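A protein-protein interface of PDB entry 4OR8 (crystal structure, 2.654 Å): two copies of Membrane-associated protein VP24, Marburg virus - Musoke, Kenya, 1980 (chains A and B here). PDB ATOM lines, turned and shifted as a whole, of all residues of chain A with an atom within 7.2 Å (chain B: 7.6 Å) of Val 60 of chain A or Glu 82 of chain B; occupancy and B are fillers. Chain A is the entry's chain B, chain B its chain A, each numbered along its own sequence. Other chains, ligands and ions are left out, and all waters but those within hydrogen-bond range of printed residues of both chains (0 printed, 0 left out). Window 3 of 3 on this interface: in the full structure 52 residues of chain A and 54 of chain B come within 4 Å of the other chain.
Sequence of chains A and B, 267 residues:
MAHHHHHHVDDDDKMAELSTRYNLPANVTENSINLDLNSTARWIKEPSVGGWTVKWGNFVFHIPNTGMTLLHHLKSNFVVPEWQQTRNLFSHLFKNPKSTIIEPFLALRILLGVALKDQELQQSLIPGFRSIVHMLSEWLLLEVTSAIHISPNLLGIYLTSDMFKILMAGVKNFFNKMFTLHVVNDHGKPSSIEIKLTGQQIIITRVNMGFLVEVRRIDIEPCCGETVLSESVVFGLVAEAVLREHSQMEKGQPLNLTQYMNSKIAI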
ATOM      1  N   GLU A  46      10.335  28.691  -4.573  1.00  0.00           N
ATOM      2  CA  GLU A  46       9.126  29.463  -4.816  1.00  0.00           C
ATOM      3  C   GLU A  46       9.115  30.728  -3.969  1.00  0.00           C
ATOM      4  O   GLU A  46       9.422  30.685  -2.776  1.00  0.00           O
ATOM      5  CB  GLU A  46       7.880  28.621  -4.541  1.00  0.00           C
ATOM      6  CG  GLU A  46       7.939  27.820  -3.250  1.00  0.00           C
ATOM      7  CD  GLU A  46       6.651  27.066  -2.978  1.00  0.00           C
ATOM      8  OE1 GLU A  46       5.606  27.451  -3.543  1.00  0.00           O
ATOM      9  OE2 GLU A  46       6.683  26.086  -2.202  1.00  0.00           O
ATOM     10  N   SER A  48       8.203  33.829  -1.640  1.00  0.00           N
ATOM     11  CA  SER A  48       7.347  33.945  -0.469  1.00  0.00           C
ATOM     12  C   SER A  48       7.593  35.271   0.233  1.00  0.00           C
ATOM     13  O   SER A  48       8.338  36.117  -0.262  1.00  0.00           O
ATOM     14  CB  SER A  48       7.569  32.775   0.495  1.00  0.00           C
ATOM     15  OG  SER A  48       8.825  32.870   1.144  1.00  0.00           O
ATOM     16  N   TRP A  52      12.173  33.813  -0.551  1.00  0.00           N
ATOM     17  CA  TRP A  52      11.823  32.551  -1.195  1.00  0.00           C
ATOM     18  C   TRP A  52      11.693  31.400  -0.212  1.00  0.00           C
ATOM     19  O   TRP A  52      12.166  31.465   0.920  1.00  0.00           O
ATOM     20  CB  TRP A  52      12.874  32.170  -2.238  1.00  0.00           C
ATOM     21  CG  TRP A  52      13.207  33.254  -3.203  1.00  0.00           C
ATOM     22  CD1 TRP A  52      12.618  33.486  -4.409  1.00  0.00           C
ATOM     23  CD2 TRP A  52      14.217  34.256  -3.047  1.00  0.00           C
ATOM     24  NE1 TRP A  52      13.200  34.571  -5.017  1.00  0.00           N
ATOM     25  CE2 TRP A  52      14.183  35.062  -4.200  1.00  0.00           C
ATOM     26  CE3 TRP A  52      15.145  34.547  -2.044  1.00  0.00           C
ATOM     27  CZ2 TRP A  52      15.043  36.144  -4.378  1.00  0.00           C
ATOM     28  CZ3 TRP A  52      15.998  35.621  -2.222  1.00  0.00           C
ATOM     29  CH2 TRP A  52      15.942  36.405  -3.382  1.00  0.00           C
ATOM     30  N   THR A  53      11.046  30.339  -0.668  1.00  0.00           N
ATOM     31  CA  THR A  53      11.042  29.082   0.055  1.00  0.00           C
ATOM     32  C   THR A  53      11.618  28.000  -0.844  1.00  0.00           C
ATOM     33  O   THR A  53      11.215  27.856  -1.998  1.00  0.00           O
ATOM     34  CB  THR A  53       9.631  28.685   0.509  1.00  0.00           C
ATOM     35  OG1 THR A  53       9.247  29.496   1.627  1.00  0.00           O
ATOM     36  CG2 THR A  53       9.593  27.225   0.924  1.00  0.00           C
ATOM     37  N   VAL A  54      12.582  27.257  -0.320  1.00  0.00           N
ATOM     38  CA  VAL A  54      13.122  26.126  -1.049  1.00  0.00           C
ATOM     39  C   VAL A  54      12.910  24.846  -0.264  1.00  0.00           C
ATOM     40  O   VAL A  54      13.321  24.734   0.892  1.00  0.00           O
ATOM     41  CB  VAL A  54      14.609  26.299  -1.362  1.00  0.00           C
ATOM     42  CG1 VAL A  54      15.125  25.077  -2.088  1.00  0.00           C
ATOM     43  CG2 VAL A  54      14.824  27.549  -2.198  1.00  0.00           C
ATOM     44  N   LYS A  55      12.247  23.889  -0.901  1.00  0.00           N
ATOM     45  CA  LYS A  55      12.020  22.586  -0.296  1.00  0.00           C
ATOM     46  C   LYS A  55      12.950  21.551  -0.900  1.00  0.00           C
ATOM     47  O   LYS A  55      13.003  21.374  -2.118  1.00  0.00           O
ATOM     48  CB  LYS A  55      10.561  22.158  -0.467  1.00  0.00           C
ATOM     49  CG  LYS A  55       9.578  23.048   0.273  1.00  0.00           C
ATOM     50  CD  LYS A  55       8.159  22.526   0.167  1.00  0.00           C
ATOM     51  CE  LYS A  55       7.197  23.417   0.937  1.00  0.00           C
ATOM     52  NZ  LYS A  55       5.808  22.886   0.921  1.00  0.00           N
ATOM     53  N   TRP A  56      13.700  20.882  -0.036  1.00  0.00           N
ATOM     54  CA  TRP A  56      14.560  19.786  -0.450  1.00  0.00           C
ATOM     55  C   TRP A  56      14.614  18.770   0.675  1.00  0.00           C
ATOM     56  O   TRP A  56      14.871  19.125   1.823  1.00  0.00           O
ATOM     57  CB  TRP A  56      15.961  20.289  -0.786  1.00  0.00           C
ATOM     58  CG  TRP A  56      16.913  19.183  -1.072  1.00  0.00           C
ATOM     59  CD1 TRP A  56      17.157  18.603  -2.280  1.00  0.00           C
ATOM     60  CD2 TRP A  56      17.743  18.505  -0.125  1.00  0.00           C
ATOM     61  NE1 TRP A  56      18.094  17.610  -2.147  1.00  0.00           N
ATOM     62  CE2 TRP A  56      18.468  17.528  -0.831  1.00  0.00           C
ATOM     63  CE3 TRP A  56      17.945  18.630   1.253  1.00  0.00           C
ATOM     64  CZ2 TRP A  56      19.383  16.682  -0.208  1.00  0.00           C
ATOM     65  CZ3 TRP A  56      18.849  17.792   1.869  1.00  0.00           C
ATOM     66  CH2 TRP A  56      19.558  16.831   1.141  1.00  0.00           C
ATOM     67  N   GLY A  57      14.374  17.506   0.346  1.00  0.00           N
ATOM     68  CA  GLY A  57      14.219  16.489   1.366  1.00  0.00           C
ATOM     69  C   GLY A  57      13.052  16.883   2.247  1.00  0.00           C
ATOM     70  O   GLY A  57      12.004  17.289   1.746  1.00  0.00           O
ATOM     71  N   ASN A  58      13.232  16.783   3.558  1.00  0.00           N
ATOM     72  CA  ASN A  58      12.214  17.248   4.492  1.00  0.00           C
ATOM     73  C   ASN A  58      12.574  18.605   5.090  1.00  0.00           C
ATOM     74  O   ASN A  58      12.054  18.990   6.136  1.00  0.00           O
ATOM     75  CB  ASN A  58      11.969  16.215   5.597  1.00  0.00           C
ATOM     76  CG  ASN A  58      13.219  15.900   6.387  1.00  0.00           C
ATOM     77  OD1 ASN A  58      14.315  16.328   6.030  1.00  0.00           O
ATOM     78  ND2 ASN A  58      13.064  15.135   7.461  1.00  0.00           N
ATOM     79  N   PHE A  59      13.472  19.323   4.422  1.00  0.00           N
ATOM     80  CA  PHE A  59      13.833  20.673   4.841  1.00  0.00           C
ATOM     81  C   PHE A  59      12.963  21.689   4.124  1.00  0.00           C
ATOM     82  O   PHE A  59      12.717  21.568   2.925  1.00  0.00           O
ATOM     83  CB  PHE A  59      15.294  20.986   4.511  1.00  0.00           C
ATOM     84  CG  PHE A  59      16.294  20.214   5.325  1.00  0.00           C
ATOM     85  CD1 PHE A  59      16.685  20.663   6.575  1.00  0.00           C
ATOM     86  CD2 PHE A  59      16.871  19.060   4.824  1.00  0.00           C
ATOM     87  CE1 PHE A  59      17.617  19.963   7.318  1.00  0.00           C
ATOM     88  CE2 PHE A  59      17.804  18.358   5.562  1.00  0.00           C
ATOM     89  CZ  PHE A  59      18.177  18.809   6.812  1.00  0.00           C
ATOM     90  N   VAL A  60      12.504  22.692   4.863  1.00  0.00           N
ATOM     91  CA  VAL A  60      11.873  23.852   4.253  1.00  0.00           C
ATOM     92  C   VAL A  60      12.732  25.078   4.542  1.00  0.00           C
ATOM     93  O   VAL A  60      12.779  25.561   5.670  1.00  0.00           O
ATOM     94  CB  VAL A  60      10.448  24.089   4.788  1.00  0.00           C
ATOM     95  CG1 VAL A  60       9.823  25.293   4.101  1.00  0.00           C
ATOM     96  CG2 VAL A  60       9.589  22.853   4.581  1.00  0.00           C
ATOM     97  N   PHE A  61      13.420  25.573   3.523  1.00  0.00           N
ATOM     98  CA  PHE A  61      14.301  26.717   3.702  1.00  0.00           C
ATOM     99  C   PHE A  61      13.575  28.039   3.472  1.00  0.00           C
ATOM    100  O   PHE A  61      12.850  28.194   2.494  1.00  0.00           O
ATOM    101  CB  PHE A  61      15.515  26.612   2.776  1.00  0.00           C
ATOM    102  CG  PHE A  61      16.420  25.456   3.092  1.00  0.00           C
ATOM    103  CD1 PHE A  61      17.211  25.472   4.227  1.00  0.00           C
ATOM    104  CD2 PHE A  61      16.488  24.358   2.249  1.00  0.00           C
ATOM    105  CE1 PHE A  61      18.050  24.414   4.522  1.00  0.00           C
ATOM    106  CE2 PHE A  61      17.325  23.295   2.537  1.00  0.00           C
ATOM    107  CZ  PHE A  61      18.107  23.325   3.675  1.00  0.00           C
ATOM    108  N   HIS A  62      13.775  28.984   4.384  1.00  0.00           N
ATOM    109  CA  HIS A  62      13.223  30.323   4.242  1.00  0.00           C
ATOM    110  C   HIS A  62      14.331  31.322   3.925  1.00  0.00           C
ATOM    111  O   HIS A  62      15.085  31.722   4.811  1.00  0.00           O
ATOM    112  CB  HIS A  62      12.493  30.738   5.515  1.00  0.00           C
ATOM    113  CG  HIS A  62      11.380  29.814   5.899  1.00  0.00           C
ATOM    114  ND1 HIS A  62      11.597  28.623   6.558  1.00  0.00           N
ATOM    115  CD2 HIS A  62      10.042  29.904   5.714  1.00  0.00           C
ATOM    116  CE1 HIS A  62      10.441  28.019   6.764  1.00  0.00           C
ATOM    117  NE2 HIS A  62       9.481  28.777   6.262  1.00  0.00           N
ATOM    118  N   ILE A  63      14.416  31.722   2.659  1.00  0.00           N
ATOM    119  CA  ILE A  63      15.487  32.597   2.191  1.00  0.00           C
ATOM    120  C   ILE A  63      15.023  34.038   2.055  1.00  0.00           C
ATOM    121  O   ILE A  63      14.145  34.330   1.246  1.00  0.00           O
ATOM    122  CB  ILE A  63      16.018  32.158   0.812  1.00  0.00           C
ATOM    123  CG1 ILE A  63      16.137  30.637   0.731  1.00  0.00           C
ATOM    124  CG2 ILE A  63      17.344  32.841   0.510  1.00  0.00           C
ATOM    125  CD1 ILE A  63      17.023  30.048   1.783  1.00  0.00           C
ATOM    126  N   VAL A 242      18.607  31.212   7.878  1.00  0.00           N
ATOM    127  CA  VAL A 242      18.352  30.127   6.936  1.00  0.00           C
ATOM    128  C   VAL A 242      18.849  28.785   7.467  1.00  0.00           C
ATOM    129  O   VAL A 242      18.162  27.768   7.363  1.00  0.00           O
ATOM    130  CB  VAL A 242      19.039  30.400   5.582  1.00  0.00           C
ATOM    131  CG1 VAL A 242      18.941  29.183   4.675  1.00  0.00           C
ATOM    132  CG2 VAL A 242      18.437  31.629   4.917  1.00  0.00           C
ATOM    133  N   GLU A 245      17.699  27.680  11.596  1.00  0.00           N
ATOM    134  CA  GLU A 245      16.425  26.981  11.682  1.00  0.00           C
ATOM    135  C   GLU A 245      16.615  25.464  11.627  1.00  0.00           C
ATOM    136  O   GLU A 245      15.799  24.711  12.152  1.00  0.00           O
ATOM    137  CB  GLU A 245      15.509  27.444  10.546  1.00  0.00           C
ATOM    138  CG  GLU A 245      14.129  26.808  10.539  1.00  0.00           C
ATOM    139  CD  GLU A 245      13.239  27.376   9.454  1.00  0.00           C
ATOM    140  OE1 GLU A 245      13.612  28.410   8.856  1.00  0.00           O
ATOM    141  OE2 GLU A 245      12.164  26.790   9.200  1.00  0.00           O
ATOM    142  N   HIS A 246      17.702  25.022  10.999  1.00  0.00           N
ATOM    143  CA  HIS A 246      17.939  23.594  10.795  1.00  0.00           C
ATOM    144  C   HIS A 246      19.300  23.129  11.311  1.00  0.00           C
ATOM    145  O   HIS A 246      19.920  22.251  10.716  1.00  0.00           O
ATOM    146  CB  HIS A 246      17.820  23.251   9.307  1.00  0.00           C
ATOM    147  CG  HIS A 246      16.552  23.737   8.678  1.00  0.00           C
ATOM    148  ND1 HIS A 246      15.333  23.131   8.895  1.00  0.00           N
ATOM    149  CD2 HIS A 246      16.314  24.771   7.837  1.00  0.00           C
ATOM    150  CE1 HIS A 246      14.399  23.772   8.215  1.00  0.00           C
ATOM    151  NE2 HIS A 246      14.967  24.771   7.565  1.00  0.00           N
ATOM    152  N   GLN A 253      10.596  26.417  15.135  1.00  0.00           N
ATOM    153  CA  GLN A 253       9.779  27.361  14.384  1.00  0.00           C
ATOM    154  C   GLN A 253      10.611  28.132  13.357  1.00  0.00           C
ATOM    155  O   GLN A 253      11.795  28.393  13.577  1.00  0.00           O
ATOM    156  CB  GLN A 253       9.092  28.342  15.333  1.00  0.00           C
ATOM    157  CG  GLN A 253      10.047  29.305  16.010  1.00  0.00           C
ATOM    158  CD  GLN A 253       9.411  30.648  16.280  1.00  0.00           C
ATOM    159  OE1 GLN A 253       8.203  30.819  16.120  1.00  0.00           O
ATOM    160  NE2 GLN A 253      10.224  31.615  16.688  1.00  0.00           N
ATOM    161  N   PRO A 254       9.989  28.503  12.223  1.00  0.00           N
ATOM    162  CA  PRO A 254      10.681  29.219  11.145  1.00  0.00           C
ATOM    163  C   PRO A 254      11.088  30.645  11.506  1.00  0.00           C
ATOM    164  O   PRO A 254      11.962  31.206  10.844  1.00  0.00           O
ATOM    165  CB  PRO A 254       9.638  29.245  10.020  1.00  0.00           C
ATOM    166  CG  PRO A 254       8.335  29.108  10.711  1.00  0.00           C
ATOM    167  CD  PRO A 254       8.600  28.180  11.852  1.00  0.00           C
ATOM    168  N   LEU B  74       2.787  38.677   9.426  1.00  0.00           N
ATOM    169  CA  LEU B  74       2.409  37.812  10.540  1.00  0.00           C
ATOM    170  C   LEU B  74       1.336  38.457  11.415  1.00  0.00           C
ATOM    171  O   LEU B  74       0.482  37.771  11.978  1.00  0.00           O
ATOM    172  CB  LEU B  74       3.638  37.465  11.384  1.00  0.00           C
ATOM    173  CG  LEU B  74       4.610  36.445  10.797  1.00  0.00           C
ATOM    174  CD1 LEU B  74       5.916  36.454  11.573  1.00  0.00           C
ATOM    175  CD2 LEU B  74       3.988  35.064  10.823  1.00  0.00           C
ATOM    176  N   VAL B  79      -0.169  35.532   5.498  1.00  0.00           N
ATOM    177  CA  VAL B  79       0.892  34.536   5.405  1.00  0.00           C
ATOM    178  C   VAL B  79       0.400  33.174   4.940  1.00  0.00           C
ATOM    179  O   VAL B  79      -0.801  32.922   4.867  1.00  0.00           O
ATOM    180  CB  VAL B  79       1.590  34.342   6.761  1.00  0.00           C
ATOM    181  CG1 VAL B  79       2.316  35.614   7.174  1.00  0.00           C
ATOM    182  CG2 VAL B  79       0.579  33.924   7.819  1.00  0.00           C
ATOM    183  N   VAL B  80       1.349  32.299   4.629  1.00  0.00           N
ATOM    184  CA  VAL B  80       1.055  30.910   4.304  1.00  0.00           C
ATOM    185  C   VAL B  80       0.887  30.122   5.606  1.00  0.00           C
ATOM    186  O   VAL B  80       1.444  30.509   6.634  1.00  0.00           O
ATOM    187  CB  VAL B  80       2.171  30.300   3.428  1.00  0.00           C
ATOM    188  CG1 VAL B  80       2.042  30.790   1.993  1.00  0.00           C
ATOM    189  CG2 VAL B  80       3.544  30.631   3.998  1.00  0.00           C
ATOM    190  N   PRO B  81       0.117  29.018   5.573  1.00  0.00           N
ATOM    191  CA  PRO B  81      -0.255  28.304   6.803  1.00  0.00           C
ATOM    192  C   PRO B  81       0.910  27.760   7.630  1.00  0.00           C
ATOM    193  O   PRO B  81       0.682  27.322   8.758  1.00  0.00           O
ATOM    194  CB  PRO B  81      -1.114  27.142   6.289  1.00  0.00           C
ATOM    195  CG  PRO B  81      -0.735  26.987   4.856  1.00  0.00           C
ATOM    196  CD  PRO B  81      -0.469  28.377   4.383  1.00  0.00           C
ATOM    197  N   GLU B  82       2.126  27.789   7.099  1.00  0.00           N
ATOM    198  CA  GLU B  82       3.274  27.264   7.832  1.00  0.00           C
ATOM    199  C   GLU B  82       3.674  28.170   8.992  1.00  0.00           C
ATOM    200  O   GLU B  82       4.475  27.782   9.840  1.00  0.00           O
ATOM    201  CB  GLU B  82       4.472  27.071   6.902  1.00  0.00           C
ATOM    202  CG  GLU B  82       5.168  28.368   6.522  1.00  0.00           C
ATOM    203  CD  GLU B  82       6.392  28.148   5.652  1.00  0.00           C
ATOM    204  OE1 GLU B  82       6.898  27.006   5.607  1.00  0.00           O
ATOM    205  OE2 GLU B  82       6.847  29.120   5.012  1.00  0.00           O
ATOM    206  N   TRP B  83       3.120  29.378   9.023  1.00  0.00           N
ATOM    207  CA  TRP B  83       3.494  30.364  10.031  1.00  0.00           C
ATOM    208  C   TRP B  83       2.487  30.445  11.171  1.00  0.00           C
ATOM    209  O   TRP B  83       2.637  31.256  12.084  1.00  0.00           O
ATOM    210  CB  TRP B  83       3.646  31.745   9.393  1.00  0.00           C
ATOM    211  CG  TRP B  83       4.806  31.859   8.451  1.00  0.00           C
ATOM    212  CD1 TRP B  83       4.779  31.716   7.096  1.00  0.00           C
ATOM    213  CD2 TRP B  83       6.164  32.152   8.797  1.00  0.00           C
ATOM    214  NE1 TRP B  83       6.038  31.898   6.576  1.00  0.00           N
ATOM    215  CE2 TRP B  83       6.906  32.168   7.599  1.00  0.00           C
ATOM    216  CE3 TRP B  83       6.825  32.403  10.004  1.00  0.00           C
ATOM    217  CZ2 TRP B  83       8.276  32.422   7.572  1.00  0.00           C
ATOM    218  CZ3 TRP B  83       8.186  32.655   9.975  1.00  0.00           C
ATOM    219  CH2 TRP B  83       8.896  32.663   8.768  1.00  0.00           C
ATOM    220  N   GLN B  84       1.462  29.601  11.115  1.00  0.00           N
ATOM    221  CA  GLN B  84       0.381  29.655  12.094  1.00  0.00           C
ATOM    222  C   GLN B  84       0.804  29.275  13.514  1.00  0.00           C
ATOM    223  O   GLN B  84       0.267  29.813  14.484  1.00  0.00           O
ATOM    224  CB  GLN B  84      -0.815  28.817  11.632  1.00  0.00           C
ATOM    225  CG  GLN B  84      -1.588  29.444  10.476  1.00  0.00           C
ATOM    226  CD  GLN B  84      -2.052  30.862  10.783  1.00  0.00           C
ATOM    227  OE1 GLN B  84      -2.478  31.163  11.899  1.00  0.00           O
ATOM    228  NE2 GLN B  84      -1.966  31.741   9.789  1.00  0.00           N
ATOM    229  N   GLN B  85       1.757  28.358  13.650  1.00  0.00           N
ATOM    230  CA  GLN B  85       2.258  27.986  14.968  1.00  0.00           C
ATOM    231  C   GLN B  85       3.136  29.098  15.530  1.00  0.00           C
ATOM    232  O   GLN B  85       3.345  29.187  16.741  1.00  0.00           O
ATOM    233  CB  GLN B  85       3.046  26.677  14.910  1.00  0.00           C
ATOM    234  CG  GLN B  85       4.358  26.776  14.151  1.00  0.00           C
ATOM    235  CD  GLN B  85       5.303  25.634  14.468  1.00  0.00           C
ATOM    236  OE1 GLN B  85       5.873  25.018  13.568  1.00  0.00           O
ATOM    237  NE2 GLN B  85       5.481  25.352  15.753  1.00  0.00           N
ATOM    238  N   THR B  86       3.651  29.941  14.640  1.00  0.00           N
ATOM    239  CA  THR B  86       4.462  31.079  15.045  1.00  0.00           C
ATOM    240  C   THR B  86       3.539  32.187  15.539  1.00  0.00           C
ATOM    241  O   THR B  86       3.809  32.825  16.558  1.00  0.00           O
ATOM    242  CB  THR B  86       5.345  31.597  13.886  1.00  0.00           C
ATOM    243  OG1 THR B  86       6.220  30.553  13.442  1.00  0.00           O
ATOM    244  CG2 THR B  86       6.181  32.785  14.339  1.00  0.00           C
ATOM    245  N   ARG B  87       2.442  32.399  14.818  1.00  0.00           N
ATOM    246  CA  ARG B  87       1.433  33.366  15.234  1.00  0.00           C
ATOM    247  C   ARG B  87       0.794  32.938  16.549  1.00  0.00           C
ATOM    248  O   ARG B  87       0.427  33.775  17.367  1.00  0.00           O
ATOM    249  CB  ARG B  87       0.353  33.537  14.160  1.00  0.00           C
ATOM    250  CG  ARG B  87       0.865  34.065  12.832  1.00  0.00           C
ATOM    251  CD  ARG B  87      -0.273  34.328  11.856  1.00  0.00           C
ATOM    252  NE  ARG B  87      -1.046  35.513  12.218  1.00  0.00           N
ATOM    253  CZ  ARG B  87      -2.239  35.484  12.804  1.00  0.00           C
ATOM    254  NH1 ARG B  87      -2.812  34.325  13.095  1.00  0.00           N
ATOM    255  NH2 ARG B  87      -2.862  36.618  13.097  1.00  0.00           N
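The side-chain carboxylate (OE2) of Glu 82 of chain B sits at hydrogen-bond distance from a ring nitrogen (NE2) of His 62 of chain A (2.9 Å).
The side-chain amide oxygen (OE1) of Gln 253 of chain A lies close to the side-chain hydroxyl (OG1) of Thr 86 of chain B (3.3 Å).
No position is printed for both chains.
Of the 6 pairs that touch across the chains among the printed residues, none has its exchanged pair printed and touching as well.
Printed residues of chain B within 4 Å of His 62 of chain A: Glu 82 and Trp 83.
Printed residues of chain B within 4 Å of Gln 253 of chain A: Thr 86 (3.3 Å).
Printed residues of chain B within 4 Å of Pro 254 of chain A: Trp 83 (3.6 Å) and Thr 86 (3.7 Å).
Pro 81 of chain B touches none of the printed residues of chain A.
Printed residues of chain A within 4 Å of Trp 83 of chain B: His 62 (3.6 Å) and Pro 254 (3.6 Å).
Of the printed residues of chain A, Thr 86 of chain B touches Gln 253 and Pro 254.
The nearest printed residue of chain B that does not touch Val 60 of chain A is Trp 83 of chain B (8.0 Å).
The nearest printed residue of chain A that does not touch Glu 82 of chain B is Thr 53 of chain A (4.2 Å).
The side-chain carboxylate of Glu 82 of chain B lies within hydrogen-bond range of the indole nitrogen of Trp 83 of chain B, 3.3 Å away.
O of Val 60 of chain A lies within hydrogen-bond range of ND1 of His 62 of chain A (3.4 Å).
The backbone carbonyl oxygen (O) of Val 60 of chain A lies within hydrogen-bond range of a ring nitrogen (NE2) of His 246 of chain A.
ND1 of His 62 of chain A lies within hydrogen-bond range of OE1 of Glu 245 of chain A (3.1 Å).
Glu 82 of chain B touches Val 60 of chain A.
His 62 of chain A touches Trp 83 of chain B (CD2 to CZ2, 3.6 Å).
Pro 254 of chain A touches Trp 83 of chain B (CG to CZ3, 3.6 Å).
Pro 254 of chain A touches Thr 86 of chain B.
Printed residues of chain A that touch a printed residue of chain B: Val 60, His 62, Gln 253 and Pro 254.
Hydrophobic or aromatic side chains of chain A within 4 Å of the printed part of chain B: Val 60, His 62 and Pro 254.
Printed residues of chain B that touch a printed residue of chain A: Glu 82, Trp 83 and Thr 86.
Hydrophobic or aromatic side chains of chain B that line the printed part of chain A: Trp 83.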
